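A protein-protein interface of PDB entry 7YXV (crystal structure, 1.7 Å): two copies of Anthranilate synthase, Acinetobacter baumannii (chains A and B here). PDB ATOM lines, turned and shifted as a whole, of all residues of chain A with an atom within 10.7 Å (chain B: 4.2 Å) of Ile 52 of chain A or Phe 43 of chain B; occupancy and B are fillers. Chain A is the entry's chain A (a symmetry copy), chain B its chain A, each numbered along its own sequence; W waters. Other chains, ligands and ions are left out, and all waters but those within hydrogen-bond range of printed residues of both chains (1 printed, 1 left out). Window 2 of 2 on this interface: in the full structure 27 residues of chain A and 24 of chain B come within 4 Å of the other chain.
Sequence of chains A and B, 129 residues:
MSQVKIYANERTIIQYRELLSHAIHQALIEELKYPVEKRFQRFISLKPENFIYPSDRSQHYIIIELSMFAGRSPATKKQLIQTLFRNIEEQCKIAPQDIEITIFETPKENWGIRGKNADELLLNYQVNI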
ATOM      1  N   TYR A   7      32.069  -9.098  -8.380  1.00  0.00           N
ATOM      2  CA  TYR A   7      32.404 -10.491  -8.600  1.00  0.00           C
ATOM      3  C   TYR A   7      32.696 -10.662 -10.110  1.00  0.00           C
ATOM      4  O   TYR A   7      31.890 -10.223 -10.932  1.00  0.00           O
ATOM      5  CB  TYR A   7      31.244 -11.393  -8.245  1.00  0.00           C
ATOM      6  CG  TYR A   7      30.833 -11.402  -6.781  1.00  0.00           C
ATOM      7  CD1 TYR A   7      30.062 -10.369  -6.274  1.00  0.00           C
ATOM      8  CD2 TYR A   7      31.107 -12.474  -5.946  1.00  0.00           C
ATOM      9  CE1 TYR A   7      29.659 -10.344  -4.946  1.00  0.00           C
ATOM     10  CE2 TYR A   7      30.701 -12.445  -4.602  1.00  0.00           C
ATOM     11  CZ  TYR A   7      29.972 -11.400  -4.148  1.00  0.00           C
ATOM     12  OH  TYR A   7      29.628 -11.431  -2.789  1.00  0.00           O
ATOM     13  N   ALA A   8      33.794 -11.352 -10.448  1.00  0.00           N
ATOM     14  CA  ALA A   8      34.185 -11.610 -11.799  1.00  0.00           C
ATOM     15  C   ALA A   8      35.151 -12.773 -11.846  1.00  0.00           C
ATOM     16  O   ALA A   8      35.760 -13.141 -10.827  1.00  0.00           O
ATOM     17  CB  ALA A   8      34.784 -10.368 -12.470  1.00  0.00           C
ATOM     18  N   ASN A   9      35.355 -13.298 -13.057  1.00  0.00           N
ATOM     19  CA  ASN A   9      36.441 -14.220 -13.293  1.00  0.00           C
ATOM     20  C   ASN A   9      37.744 -13.579 -12.999  1.00  0.00           C
ATOM     21  O   ASN A   9      37.937 -12.361 -13.227  1.00  0.00           O
ATOM     22  CB  ASN A   9      36.404 -14.764 -14.733  1.00  0.00           C
ATOM     23  CG  ASN A   9      35.215 -15.610 -15.034  1.00  0.00           C
ATOM     24  OD1 ASN A   9      35.006 -16.649 -14.357  1.00  0.00           O
ATOM     25  ND2 ASN A   9      34.424 -15.245 -16.095  1.00  0.00           N
ATOM     26  N   ILE A  44      35.937  -9.700  -5.809  1.00  0.00           N
ATOM     27  CA  ILE A  44      35.810 -11.095  -5.474  1.00  0.00           C
ATOM     28  C   ILE A  44      36.201 -11.910  -6.726  1.00  0.00           C
ATOM     29  O   ILE A  44      35.457 -11.972  -7.708  1.00  0.00           O
ATOM     30  CB  ILE A  44      34.398 -11.484  -4.964  1.00  0.00           C
ATOM     31  CG1 ILE A  44      33.903 -10.576  -3.833  1.00  0.00           C
ATOM     32  CG2 ILE A  44      34.451 -12.937  -4.562  1.00  0.00           C
ATOM     33  CD1 ILE A  44      34.837 -10.509  -2.604  1.00  0.00           C
ATOM     34  N   SER A  45      37.421 -12.396  -6.716  1.00  0.00           N
ATOM     35  CA  SER A  45      38.080 -12.992  -7.848  1.00  0.00           C
ATOM     36  C   SER A  45      37.800 -14.468  -7.902  1.00  0.00           C
ATOM     37  O   SER A  45      38.279 -15.211  -7.009  1.00  0.00           O
ATOM     38  CB  SER A  45      39.564 -12.687  -7.715  1.00  0.00           C
ATOM     39  OG  SER A  45      40.248 -13.237  -8.824  1.00  0.00           O
ATOM     40  N   LEU A  46      37.027 -14.902  -8.882  1.00  0.00           N
ATOM     41  CA  LEU A  46      36.551 -16.277  -8.930  1.00  0.00           C
ATOM     42  C   LEU A  46      37.273 -17.085 -10.022  1.00  0.00           C
ATOM     43  O   LEU A  46      37.452 -16.601 -11.126  1.00  0.00           O
ATOM     44  CB  LEU A  46      35.030 -16.321  -9.259  1.00  0.00           C
ATOM     45  CG  LEU A  46      34.166 -15.616  -8.172  1.00  0.00           C
ATOM     46  CD1 LEU A  46      32.741 -15.554  -8.650  1.00  0.00           C
ATOM     47  CD2 LEU A  46      34.288 -16.295  -6.860  1.00  0.00           C
ATOM     48  N   LYS A  47      37.640 -18.310  -9.718  1.00  0.00           N
ATOM     49  CA  LYS A  47      38.072 -19.282 -10.747  1.00  0.00           C
ATOM     50  C   LYS A  47      36.878 -19.587 -11.604  1.00  0.00           C
ATOM     51  O   LYS A  47      35.762 -19.727 -11.133  1.00  0.00           O
ATOM     52  CB  LYS A  47      38.559 -20.601 -10.158  1.00  0.00           C
ATOM     53  CG  LYS A  47      39.808 -20.472  -9.344  1.00  0.00           C
ATOM     54  CD  LYS A  47      39.972 -21.648  -8.389  1.00  0.00           C
ATOM     55  CE  LYS A  47      41.282 -21.508  -7.645  1.00  0.00           C
ATOM     56  NZ  LYS A  47      41.333 -22.682  -6.786  1.00  0.00           N
ATOM     57  N   PRO A  48      37.075 -19.708 -12.936  1.00  0.00           N
ATOM     58  CA  PRO A  48      35.902 -19.849 -13.748  1.00  0.00           C
ATOM     59  C   PRO A  48      35.019 -21.040 -13.431  1.00  0.00           C
ATOM     60  O   PRO A  48      33.773 -20.996 -13.608  1.00  0.00           O
ATOM     61  CB  PRO A  48      36.487 -19.910 -15.214  1.00  0.00           C
ATOM     62  CG  PRO A  48      37.829 -19.485 -15.085  1.00  0.00           C
ATOM     63  CD  PRO A  48      38.308 -19.533 -13.683  1.00  0.00           C
ATOM     64  N   GLU A  49      35.618 -22.115 -12.951  1.00  0.00           N
ATOM     65  CA  GLU A  49      34.821 -23.296 -12.621  1.00  0.00           C
ATOM     66  C   GLU A  49      33.820 -23.048 -11.508  1.00  0.00           C
ATOM     67  O   GLU A  49      32.826 -23.771 -11.419  1.00  0.00           O
ATOM     68  CB  GLU A  49      35.705 -24.517 -12.231  1.00  0.00           C
ATOM     69  CG  GLU A  49      36.714 -24.273 -11.145  1.00  0.00           C
ATOM     70  CD  GLU A  49      38.088 -23.751 -11.641  1.00  0.00           C
ATOM     71  OE1 GLU A  49      38.246 -23.097 -12.758  1.00  0.00           O
ATOM     72  OE2 GLU A  49      39.054 -24.016 -10.853  1.00  0.00           O
ATOM     73  N   ASN A  50      34.041 -21.979 -10.726  1.00  0.00           N
ATOM     74  CA  ASN A  50      33.170 -21.627  -9.615  1.00  0.00           C
ATOM     75  C   ASN A  50      32.207 -20.503  -9.966  1.00  0.00           C
ATOM     76  O   ASN A  50      31.398 -20.070  -9.118  1.00  0.00           O
ATOM     77  CB  ASN A  50      34.087 -21.191  -8.424  1.00  0.00           C
ATOM     78  CG  ASN A  50      34.752 -22.372  -7.838  1.00  0.00           C
ATOM     79  OD1 ASN A  50      34.199 -23.481  -7.826  1.00  0.00           O
ATOM     80  ND2 ASN A  50      35.949 -22.170  -7.347  1.00  0.00           N
ATOM     81  N   PHE A  51      32.220 -20.084 -11.241  1.00  0.00           N
ATOM     82  CA  PHE A  51      31.397 -18.899 -11.644  1.00  0.00           C
ATOM     83  C   PHE A  51      30.566 -19.374 -12.855  1.00  0.00           C
ATOM     84  O   PHE A  51      31.084 -19.457 -13.979  1.00  0.00           O
ATOM     85  CB  PHE A  51      32.243 -17.694 -11.975  1.00  0.00           C
ATOM     86  CG  PHE A  51      31.479 -16.440 -12.153  1.00  0.00           C
ATOM     87  CD1 PHE A  51      30.151 -16.257 -11.742  1.00  0.00           C
ATOM     88  CD2 PHE A  51      32.127 -15.330 -12.763  1.00  0.00           C
ATOM     89  CE1 PHE A  51      29.515 -15.024 -11.940  1.00  0.00           C
ATOM     90  CE2 PHE A  51      31.488 -14.140 -12.932  1.00  0.00           C
ATOM     91  CZ  PHE A  51      30.230 -13.967 -12.508  1.00  0.00           C
ATOM     92  N   ILE A  52      29.332 -19.824 -12.594  1.00  0.00           N
ATOM     93  CA  ILE A  52      28.493 -20.521 -13.586  1.00  0.00           C
ATOM     94  C   ILE A  52      27.316 -19.626 -14.027  1.00  0.00           C
ATOM     95  O   ILE A  52      26.582 -19.115 -13.187  1.00  0.00           O
ATOM     96  CB  ILE A  52      27.984 -21.815 -12.933  1.00  0.00           C
ATOM     97  CG1 ILE A  52      29.153 -22.744 -12.623  1.00  0.00           C
ATOM     98  CG2 ILE A  52      26.877 -22.500 -13.763  1.00  0.00           C
ATOM     99  CD1 ILE A  52      28.745 -23.960 -11.837  1.00  0.00           C
ATOM    100  N   TYR A  53      27.229 -19.320 -15.325  1.00  0.00           N
ATOM    101  CA  TYR A  53      26.245 -18.389 -15.815  1.00  0.00           C
ATOM    102  C   TYR A  53      26.042 -18.695 -17.277  1.00  0.00           C
ATOM    103  O   TYR A  53      26.852 -19.463 -17.853  1.00  0.00           O
ATOM    104  CB  TYR A  53      26.733 -16.965 -15.584  1.00  0.00           C
ATOM    105  CG  TYR A  53      28.080 -16.657 -16.112  1.00  0.00           C
ATOM    106  CD1 TYR A  53      28.241 -16.175 -17.426  1.00  0.00           C
ATOM    107  CD2 TYR A  53      29.254 -16.798 -15.336  1.00  0.00           C
ATOM    108  CE1 TYR A  53      29.482 -15.857 -17.940  1.00  0.00           C
ATOM    109  CE2 TYR A  53      30.478 -16.413 -15.830  1.00  0.00           C
ATOM    110  CZ  TYR A  53      30.606 -15.964 -17.115  1.00  0.00           C
ATOM    111  OH  TYR A  53      31.854 -15.564 -17.584  1.00  0.00           O
ATOM    112  N   PRO A  54      24.969 -18.149 -17.862  1.00  0.00           N
ATOM    113  CA  PRO A  54      24.638 -18.508 -19.254  1.00  0.00           C
ATOM    114  C   PRO A  54      25.698 -18.102 -20.264  1.00  0.00           C
ATOM    115  O   PRO A  54      26.408 -17.075 -20.081  1.00  0.00           O
ATOM    116  CB  PRO A  54      23.283 -17.802 -19.489  1.00  0.00           C
ATOM    117  CG  PRO A  54      22.727 -17.611 -18.126  1.00  0.00           C
ATOM    118  CD  PRO A  54      23.921 -17.328 -17.252  1.00  0.00           C
ATOM    119  N   SER A  55      25.786 -18.845 -21.385  1.00  0.00           N
ATOM    120  CA  SER A  55      26.775 -18.628 -22.391  1.00  0.00           C
ATOM    121  C   SER A  55      26.585 -17.373 -23.222  1.00  0.00           C
ATOM    122  O   SER A  55      27.526 -16.991 -23.948  1.00  0.00           O
ATOM    123  CB  SER A  55      26.795 -19.827 -23.372  1.00  0.00           C
ATOM    124  OG  SER A  55      25.513 -19.914 -23.960  1.00  0.00           O
ATOM    125  N   ASP A  56      25.428 -16.728 -23.104  1.00  0.00           N
ATOM    126  CA  ASP A  56      25.202 -15.384 -23.681  1.00  0.00           C
ATOM    127  C   ASP A  56      25.748 -14.197 -22.917  1.00  0.00           C
ATOM    128  O   ASP A  56      25.578 -13.043 -23.334  1.00  0.00           O
ATOM    129  CB  ASP A  56      23.699 -15.209 -24.022  1.00  0.00           C
ATOM    130  CG  ASP A  56      22.807 -15.068 -22.795  1.00  0.00           C
ATOM    131  OD1 ASP A  56      23.300 -15.156 -21.680  1.00  0.00           O
ATOM    132  OD2 ASP A  56      21.564 -15.040 -22.961  1.00  0.00           O
ATOM    133  N   ARG A  57      26.465 -14.453 -21.816  1.00  0.00           N
ATOM    134  CA  ARG A  57      27.319 -13.441 -21.241  1.00  0.00           C
ATOM    135  C   ARG A  57      28.778 -13.965 -21.506  1.00  0.00           C
ATOM    136  O   ARG A  57      29.022 -15.198 -21.442  1.00  0.00           O
ATOM    137  CB  ARG A  57      27.083 -13.289 -19.743  1.00  0.00           C
ATOM    138  CG  ARG A  57      25.849 -12.528 -19.383  1.00  0.00           C
ATOM    139  CD  ARG A  57      24.643 -13.356 -19.264  1.00  0.00           C
ATOM    140  NE  ARG A  57      23.554 -12.692 -18.536  1.00  0.00           N
ATOM    141  CZ  ARG A  57      22.272 -12.980 -18.692  1.00  0.00           C
ATOM    142  NH1 ARG A  57      21.888 -13.878 -19.555  1.00  0.00           N
ATOM    143  NH2 ARG A  57      21.350 -12.335 -18.001  1.00  0.00           N
ATOM    144  N   SER A  58      29.708 -13.042 -21.685  1.00  0.00           N
ATOM    145  CA  SER A  58      31.067 -13.402 -22.095  1.00  0.00           C
ATOM    146  C   SER A  58      31.943 -13.767 -20.869  1.00  0.00           C
ATOM    147  O   SER A  58      31.485 -13.791 -19.737  1.00  0.00           O
ATOM    148  CB  SER A  58      31.732 -12.296 -22.898  1.00  0.00           C
ATOM    149  OG  SER A  58      32.264 -11.241 -22.080  1.00  0.00           O
ATOM    150  N   GLN A  59      33.213 -14.024 -21.140  1.00  0.00           N
ATOM    151  CA  GLN A  59      34.222 -14.172 -20.059  1.00  0.00           C
ATOM    152  C   GLN A  59      34.247 -12.930 -19.126  1.00  0.00           C
ATOM    153  O   GLN A  59      34.701 -13.041 -18.030  1.00  0.00           O
ATOM    154  CB  GLN A  59      35.612 -14.433 -20.641  1.00  0.00           C
ATOM    155  CG  GLN A  59      36.169 -13.306 -21.481  1.00  0.00           C
ATOM    156  CD  GLN A  59      35.849 -13.460 -22.949  1.00  0.00           C
ATOM    157  OE1 GLN A  59      34.756 -13.900 -23.350  1.00  0.00           O
ATOM    158  NE2 GLN A  59      36.831 -13.027 -23.786  1.00  0.00           N
ATOM    159  N   TYR A  61      31.692 -11.281 -17.820  1.00  0.00           N
ATOM    160  CA  TYR A  61      30.492 -11.128 -16.981  1.00  0.00           C
ATOM    161  C   TYR A  61      30.907 -10.659 -15.580  1.00  0.00           C
ATOM    162  O   TYR A  61      31.792 -11.273 -14.935  1.00  0.00           O
ATOM    163  CB  TYR A  61      29.695 -12.464 -16.911  1.00  0.00           C
ATOM    164  CG  TYR A  61      28.454 -12.442 -16.095  1.00  0.00           C
ATOM    165  CD1 TYR A  61      27.466 -11.435 -16.243  1.00  0.00           C
ATOM    166  CD2 TYR A  61      28.226 -13.438 -15.157  1.00  0.00           C
ATOM    167  CE1 TYR A  61      26.289 -11.466 -15.478  1.00  0.00           C
ATOM    168  CE2 TYR A  61      27.080 -13.493 -14.399  1.00  0.00           C
ATOM    169  CZ  TYR A  61      26.118 -12.495 -14.547  1.00  0.00           C
ATOM    170  OH  TYR A  61      25.024 -12.574 -13.769  1.00  0.00           O
ATOM    171  N   ILE A  62      30.284  -9.564 -15.136  1.00  0.00           N
ATOM    172  CA  ILE A  62      30.610  -8.933 -13.847  1.00  0.00           C
ATOM    173  C   ILE A  62      29.307  -8.713 -13.092  1.00  0.00           C
ATOM    174  O   ILE A  62      28.345  -8.203 -13.638  1.00  0.00           O
ATOM    175  CB  ILE A  62      31.428  -7.638 -13.949  1.00  0.00           C
ATOM    176  CG1 ILE A  62      30.642  -6.448 -14.518  1.00  0.00           C
ATOM    177  CG2 ILE A  62      32.700  -7.893 -14.734  1.00  0.00           C
ATOM    178  CD1 ILE A  62      31.505  -5.216 -14.638  1.00  0.00           C
ATOM    179  N   ILE A  63      29.295  -9.065 -11.777  1.00  0.00           N
ATOM    180  CA  ILE A  63      28.181  -8.795 -10.902  1.00  0.00           C
ATOM    181  C   ILE A  63      28.637  -7.776  -9.866  1.00  0.00           C
ATOM    182  O   ILE A  63      29.587  -8.116  -9.114  1.00  0.00           O
ATOM    183  CB  ILE A  63      27.711 -10.077 -10.181  1.00  0.00           C
ATOM    184  CG1 ILE A  63      27.149 -11.100 -11.251  1.00  0.00           C
ATOM    185  CG2 ILE A  63      26.606  -9.761  -9.168  1.00  0.00           C
ATOM    186  CD1 ILE A  63      26.874 -12.469 -10.689  1.00  0.00           C
ATOM    187  N   GLU A 100      25.978  -6.849 -14.542  1.00  0.00           N
ATOM    188  CA  GLU A 100      24.792  -6.990 -13.724  1.00  0.00           C
ATOM    189  C   GLU A 100      24.973  -6.319 -12.383  1.00  0.00           C
ATOM    190  O   GLU A 100      26.063  -6.346 -11.854  1.00  0.00           O
ATOM    191  CB  GLU A 100      24.462  -8.495 -13.540  1.00  0.00           C
ATOM    192  CG  GLU A 100      23.178  -8.690 -12.830  1.00  0.00           C
ATOM    193  CD  GLU A 100      22.752 -10.123 -12.722  1.00  0.00           C
ATOM    194  OE1 GLU A 100      22.939 -10.917 -13.688  1.00  0.00           O
ATOM    195  OE2 GLU A 100      22.272 -10.479 -11.596  1.00  0.00           O
ATOM    196  N   ILE B   6      26.938 -20.131  -3.149  1.00  0.00           N
ATOM    197  CA  ILE B   6      27.043 -21.391  -2.429  1.00  0.00           C
ATOM    198  C   ILE B   6      28.418 -21.372  -1.728  1.00  0.00           C
ATOM    199  O   ILE B   6      29.450 -21.317  -2.394  1.00  0.00           O
ATOM    200  CB  ILE B   6      26.980 -22.609  -3.372  1.00  0.00           C
ATOM    201  CG1 ILE B   6      25.711 -22.588  -4.255  1.00  0.00           C
ATOM    202  CG2 ILE B   6      27.069 -23.874  -2.547  1.00  0.00           C
ATOM    203  CD1 ILE B   6      25.866 -21.889  -5.589  1.00  0.00           C
ATOM    204  N   ARG B  17      30.313 -29.747  -6.623  1.00  0.00           N
ATOM    205  CA  ARG B  17      29.862 -28.561  -7.279  1.00  0.00           C
ATOM    206  C   ARG B  17      28.840 -28.913  -8.362  1.00  0.00           C
ATOM    207  O   ARG B  17      27.821 -28.245  -8.492  1.00  0.00           O
ATOM    208  CB  ARG B  17      31.040 -27.888  -7.954  1.00  0.00           C
ATOM    209  CG  ARG B  17      30.652 -26.592  -8.686  1.00  0.00           C
ATOM    210  CD  ARG B  17      31.771 -26.176  -9.609  1.00  0.00           C
ATOM    211  NE  ARG B  17      33.046 -25.879  -8.963  1.00  0.00           N
ATOM    212  CZ  ARG B  17      34.170 -26.588  -9.079  1.00  0.00           C
ATOM    213  NH1 ARG B  17      34.233 -27.750  -9.750  1.00  0.00           N
ATOM    214  NH2 ARG B  17      35.242 -26.217  -8.439  1.00  0.00           N
ATOM    215  N   LEU B  20      25.541 -30.212  -6.901  1.00  0.00           N
ATOM    216  CA  LEU B  20      24.809 -29.098  -6.242  1.00  0.00           C
ATOM    217  C   LEU B  20      24.248 -28.171  -7.312  1.00  0.00           C
ATOM    218  O   LEU B  20      23.094 -27.724  -7.166  1.00  0.00           O
ATOM    219  CB  LEU B  20      25.750 -28.292  -5.330  1.00  0.00           C
ATOM    220  CG  LEU B  20      26.048 -28.978  -4.000  1.00  0.00           C
ATOM    221  CD1 LEU B  20      27.221 -28.327  -3.314  1.00  0.00           C
ATOM    222  CD2 LEU B  20      24.839 -28.900  -3.089  1.00  0.00           C
ATOM    223  N   SER B  21      25.012 -27.855  -8.344  1.00  0.00           N
ATOM    224  CA  SER B  21      24.586 -26.936  -9.340  1.00  0.00           C
ATOM    225  C   SER B  21      23.260 -27.403  -9.972  1.00  0.00           C
ATOM    226  O   SER B  21      22.312 -26.647 -10.153  1.00  0.00           O
ATOM    227  CB  SER B  21      25.644 -26.814 -10.453  1.00  0.00           C
ATOM    228  OG  SER B  21      25.239 -25.880 -11.470  1.00  0.00           O
ATOM    229  N   ARG B  39      20.514 -20.107 -15.187  1.00  0.00           N
ATOM    230  CA  ARG B  39      21.279 -20.552 -13.990  1.00  0.00           C
ATOM    231  C   ARG B  39      22.488 -19.676 -13.705  1.00  0.00           C
ATOM    232  O   ARG B  39      23.381 -19.503 -14.543  1.00  0.00           O
ATOM    233  CB  ARG B  39      21.693 -21.968 -14.116  1.00  0.00           C
ATOM    234  CG  ARG B  39      22.947 -22.368 -13.402  1.00  0.00           C
ATOM    235  CD  ARG B  39      23.585 -23.464 -14.188  1.00  0.00           C
ATOM    236  NE  ARG B  39      22.769 -24.639 -14.081  1.00  0.00           N
ATOM    237  CZ  ARG B  39      22.993 -25.747 -14.734  1.00  0.00           C
ATOM    238  NH1 ARG B  39      22.204 -26.802 -14.510  1.00  0.00           N
ATOM    239  NH2 ARG B  39      23.994 -25.791 -15.611  1.00  0.00           N
ATOM    240  N   PHE B  40      22.457 -19.075 -12.519  1.00  0.00           N
ATOM    241  CA  PHE B  40      23.475 -18.078 -12.140  1.00  0.00           C
ATOM    242  C   PHE B  40      23.961 -18.446 -10.742  1.00  0.00           C
ATOM    243  O   PHE B  40      23.200 -18.244  -9.791  1.00  0.00           O
ATOM    244  CB  PHE B  40      22.867 -16.690 -12.083  1.00  0.00           C
ATOM    245  CG  PHE B  40      22.361 -16.178 -13.423  1.00  0.00           C
ATOM    246  CD1 PHE B  40      21.090 -16.508 -13.853  1.00  0.00           C
ATOM    247  CD2 PHE B  40      23.150 -15.301 -14.197  1.00  0.00           C
ATOM    248  CE1 PHE B  40      20.604 -16.022 -15.080  1.00  0.00           C
ATOM    249  CE2 PHE B  40      22.671 -14.843 -15.405  1.00  0.00           C
ATOM    250  CZ  PHE B  40      21.413 -15.188 -15.831  1.00  0.00           C
ATOM    251  N   GLN B  41      25.141 -19.028 -10.670  1.00  0.00           N
ATOM    252  CA  GLN B  41      25.701 -19.567  -9.417  1.00  0.00           C
ATOM    253  C   GLN B  41      27.153 -19.181  -9.226  1.00  0.00           C
ATOM    254  O   GLN B  41      27.971 -19.251 -10.188  1.00  0.00           O
ATOM    255  CB  GLN B  41      25.596 -21.102  -9.448  1.00  0.00           C
ATOM    256  CG  GLN B  41      24.167 -21.588  -9.658  1.00  0.00           C
ATOM    257  CD  GLN B  41      24.066 -23.056  -9.832  1.00  0.00           C
ATOM    258  OE1 GLN B  41      25.068 -23.666 -10.134  1.00  0.00           O
ATOM    259  NE2 GLN B  41      22.780 -23.634  -9.804  1.00  0.00           N
ATOM    260  N   ARG B  42      27.490 -18.749  -7.997  1.00  0.00           N
ATOM    261  CA  ARG B  42      28.846 -18.489  -7.628  1.00  0.00           C
ATOM    262  C   ARG B  42      29.157 -19.435  -6.427  1.00  0.00           C
ATOM    263  O   ARG B  42      28.494 -19.361  -5.398  1.00  0.00           O
ATOM    264  CB  ARG B  42      29.008 -17.056  -7.164  1.00  0.00           C
ATOM    265  CG  ARG B  42      29.143 -16.064  -8.325  1.00  0.00           C
ATOM    266  CD  ARG B  42      28.892 -14.625  -7.931  1.00  0.00           C
ATOM    267  NE  ARG B  42      27.439 -14.447  -7.729  1.00  0.00           N
ATOM    268  CZ  ARG B  42      26.868 -13.385  -7.221  1.00  0.00           C
ATOM    269  NH1 ARG B  42      27.578 -12.375  -6.750  1.00  0.00           N
ATOM    270  NH2 ARG B  42      25.568 -13.305  -7.156  1.00  0.00           N
ATOM    271  N   PHE B  43      30.138 -20.279  -6.611  1.00  0.00           N
ATOM    272  CA  PHE B  43      30.619 -21.205  -5.533  1.00  0.00           C
ATOM    273  C   PHE B  43      31.808 -20.486  -4.868  1.00  0.00           C
ATOM    274  O   PHE B  43      32.801 -20.149  -5.533  1.00  0.00           O
ATOM    275  CB  PHE B  43      31.025 -22.534  -6.108  1.00  0.00           C
ATOM    276  CG  PHE B  43      29.826 -23.347  -6.552  1.00  0.00           C
ATOM    277  CD1 PHE B  43      29.288 -23.182  -7.840  1.00  0.00           C
ATOM    278  CD2 PHE B  43      29.273 -24.303  -5.703  1.00  0.00           C
ATOM    279  CE1 PHE B  43      28.122 -23.901  -8.236  1.00  0.00           C
ATOM    280  CE2 PHE B  43      28.141 -24.976  -6.104  1.00  0.00           C
ATOM    281  CZ  PHE B  43      27.605 -24.769  -7.400  1.00  0.00           C
ATOM    282  N   ILE B  44      31.653 -20.239  -3.577  1.00  0.00           N
ATOM    283  CA  ILE B  44      32.600 -19.541  -2.746  1.00  0.00           C
ATOM    284  C   ILE B  44      33.370 -20.600  -1.929  1.00  0.00           C
ATOM    285  O   ILE B  44      32.836 -21.200  -0.992  1.00  0.00           O
ATOM    286  CB  ILE B  44      31.948 -18.477  -1.825  1.00  0.00           C
ATOM    287  CG1 ILE B  44      31.031 -17.513  -2.584  1.00  0.00           C
ATOM    288  CG2 ILE B  44      33.066 -17.768  -1.100  1.00  0.00           C
ATOM    289  CD1 ILE B  44      31.710 -16.760  -3.751  1.00  0.00           C
ATOM    290  N   SER B  45      34.559 -20.906  -2.394  1.00  0.00           N
ATOM    291  CA  SER B  45      35.364 -22.008  -1.938  1.00  0.00           C
ATOM    292  C   SER B  45      36.237 -21.584  -0.790  1.00  0.00           C
ATOM    293  O   SER B  45      37.166 -20.766  -1.004  1.00  0.00           O
ATOM    294  CB  SER B  45      36.170 -22.500  -3.131  1.00  0.00           C
ATOM    295  OG  SER B  45      36.959 -23.603  -2.731  1.00  0.00           O
HETATM  296  O   HOH W   1      26.593 -16.266 -11.723  1.00  0.00           O
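NE of Arg 17 of chain B sits close to O of Glu 49 of chain A. The side-chain amide oxygen (OD1) of Asn 50 of chain A lies within hydrogen-bond range of the guanidinium group (NE) of Arg 17 of chain B (2.9 Å). The backbone carbonyl oxygen (O) of Gln 41 of chain B sits at hydrogen-bond distance from the backbone NH (N) of Ile 52 of chain A, at 2.8 Å. O of Asn 50 of chain A is in hydrogen-bond range of N of Phe 43 of chain B (2.8 Å). O of Ile 52 of chain A sits close to O of Arg 39 of chain B (3.5 Å).
The side-chain hydroxyl of Ser 21 of chain B sits at hydrogen-bond distance from the side-chain amide oxygen of Gln 41 of chain B (2.6 Å). O of Ala 8 of chain A lies within hydrogen-bond range of N of Leu 46 of chain A (2.9 Å). The side-chain amide nitrogen of Asn 9 of chain A sits at hydrogen-bond distance from the side-chain hydroxyl of Tyr 53 of chain A. OH of Tyr 53 of chain A sits at hydrogen-bond distance from O of Ser 58 of chain A, at 2.8 Å. The guanidinium group (NH1) of Arg 57 of chain A lies within salt-bridge range of the side-chain carboxylate (OD1) of Asp 56 of chain A (2.9 Å). The side-chain hydroxyl (OH) of Tyr 61 of chain A sits at hydrogen-bond distance from the side-chain carboxylate (OE1) of Glu 100 of chain A (2.7 Å).
Among the printed residues, merely in contact across the chains: Tyr 7 of chain A with Arg 42 of chain B, Leu 46 of chain A with Arg 42 of chain B, Asn 50 of chain A with Gln 41 of chain B, Asn 50 of chain A with Arg 42 of chain B, Phe 51 of chain A with Gln 41 of chain B, Phe 51 of chain A with Arg 42 of chain B, Ile 52 of chain A with Phe 40 of chain B, Ile 52 of chain A with Phe 43 of chain B, Tyr 53 of chain A with Arg 39 of chain B, Pro 54 of chain A with Arg 39 of chain B, Pro 54 of chain A with Phe 40 of chain B, Arg 57 of chain A with Phe 40 of chain B, Tyr 61 of chain A with Phe 40 of chain B and Ile 63 of chain A with Arg 42 of chain B.
Printed residues of chain B within 4 Å of Ile 52 of chain A: Arg 39, Phe 40, Gln 41 and Phe 43. Phe 43 of chain B touches just these residues of chain A: Asn 50 (2.8 Å) and Ile 52 (3.7 Å). Ile 6 of chain B touches none of the printed residues of chain A. No residue of chain A comes within 4 Å of Leu 20 of chain B. No residue of chain A comes within 4 Å of Ile 44 of chain B. No residue of chain A comes within 4 Å of Ser 45 of chain B. Of the printed residues of chain A, Arg 39 of chain B touches Ile 52 (3.5 Å), Tyr 53 (3.3 Å) and Pro 54 (3.5 Å). Of the printed residues of chain B, Tyr 61 of chain A touches Phe 40. Of the printed residues of chain A, Phe 40 of chain B touches Ile 52 (3.4 Å), Pro 54 (3.3 Å), Arg 57 (3.6 Å) and Tyr 61 (3.3 Å). Of the printed residues of chain B, Pro 54 of chain A touches Arg 39 (3.5 Å) and Phe 40 (3.3 Å). The nearest printed residue of chain B that does not touch Ile 52 of chain A is Ser 21 of chain B (4.01 Å).
Hydrophobic or aromatic side chains of chain A that line the printed part of chain B: Tyr 7, Leu 46, Phe 51, Ile 52, Pro 54, Tyr 61 and Ile 63. Printed residues of chain B that touch a printed residue of chain A: Arg 17, Arg 39, Phe 40, Gln 41, Arg 42 and Phe 43. Among the printed residues, 19 pairs touch across the chains. Among the printed residues, no Asp or Glu carboxylate lies within 4 Å of a Lys or Arg side-chain nitrogen of the other chain.
Positions printed for both chains: 44 and 45. Of the 19 pairs that touch across the chains among the printed residues, none has its exchanged pair printed and touching as well.
Water W1 lies within hydrogen-bond range of O of Ile 52 of chain A (3.2 Å) and N of Gln 41 of chain B (3.3 Å).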
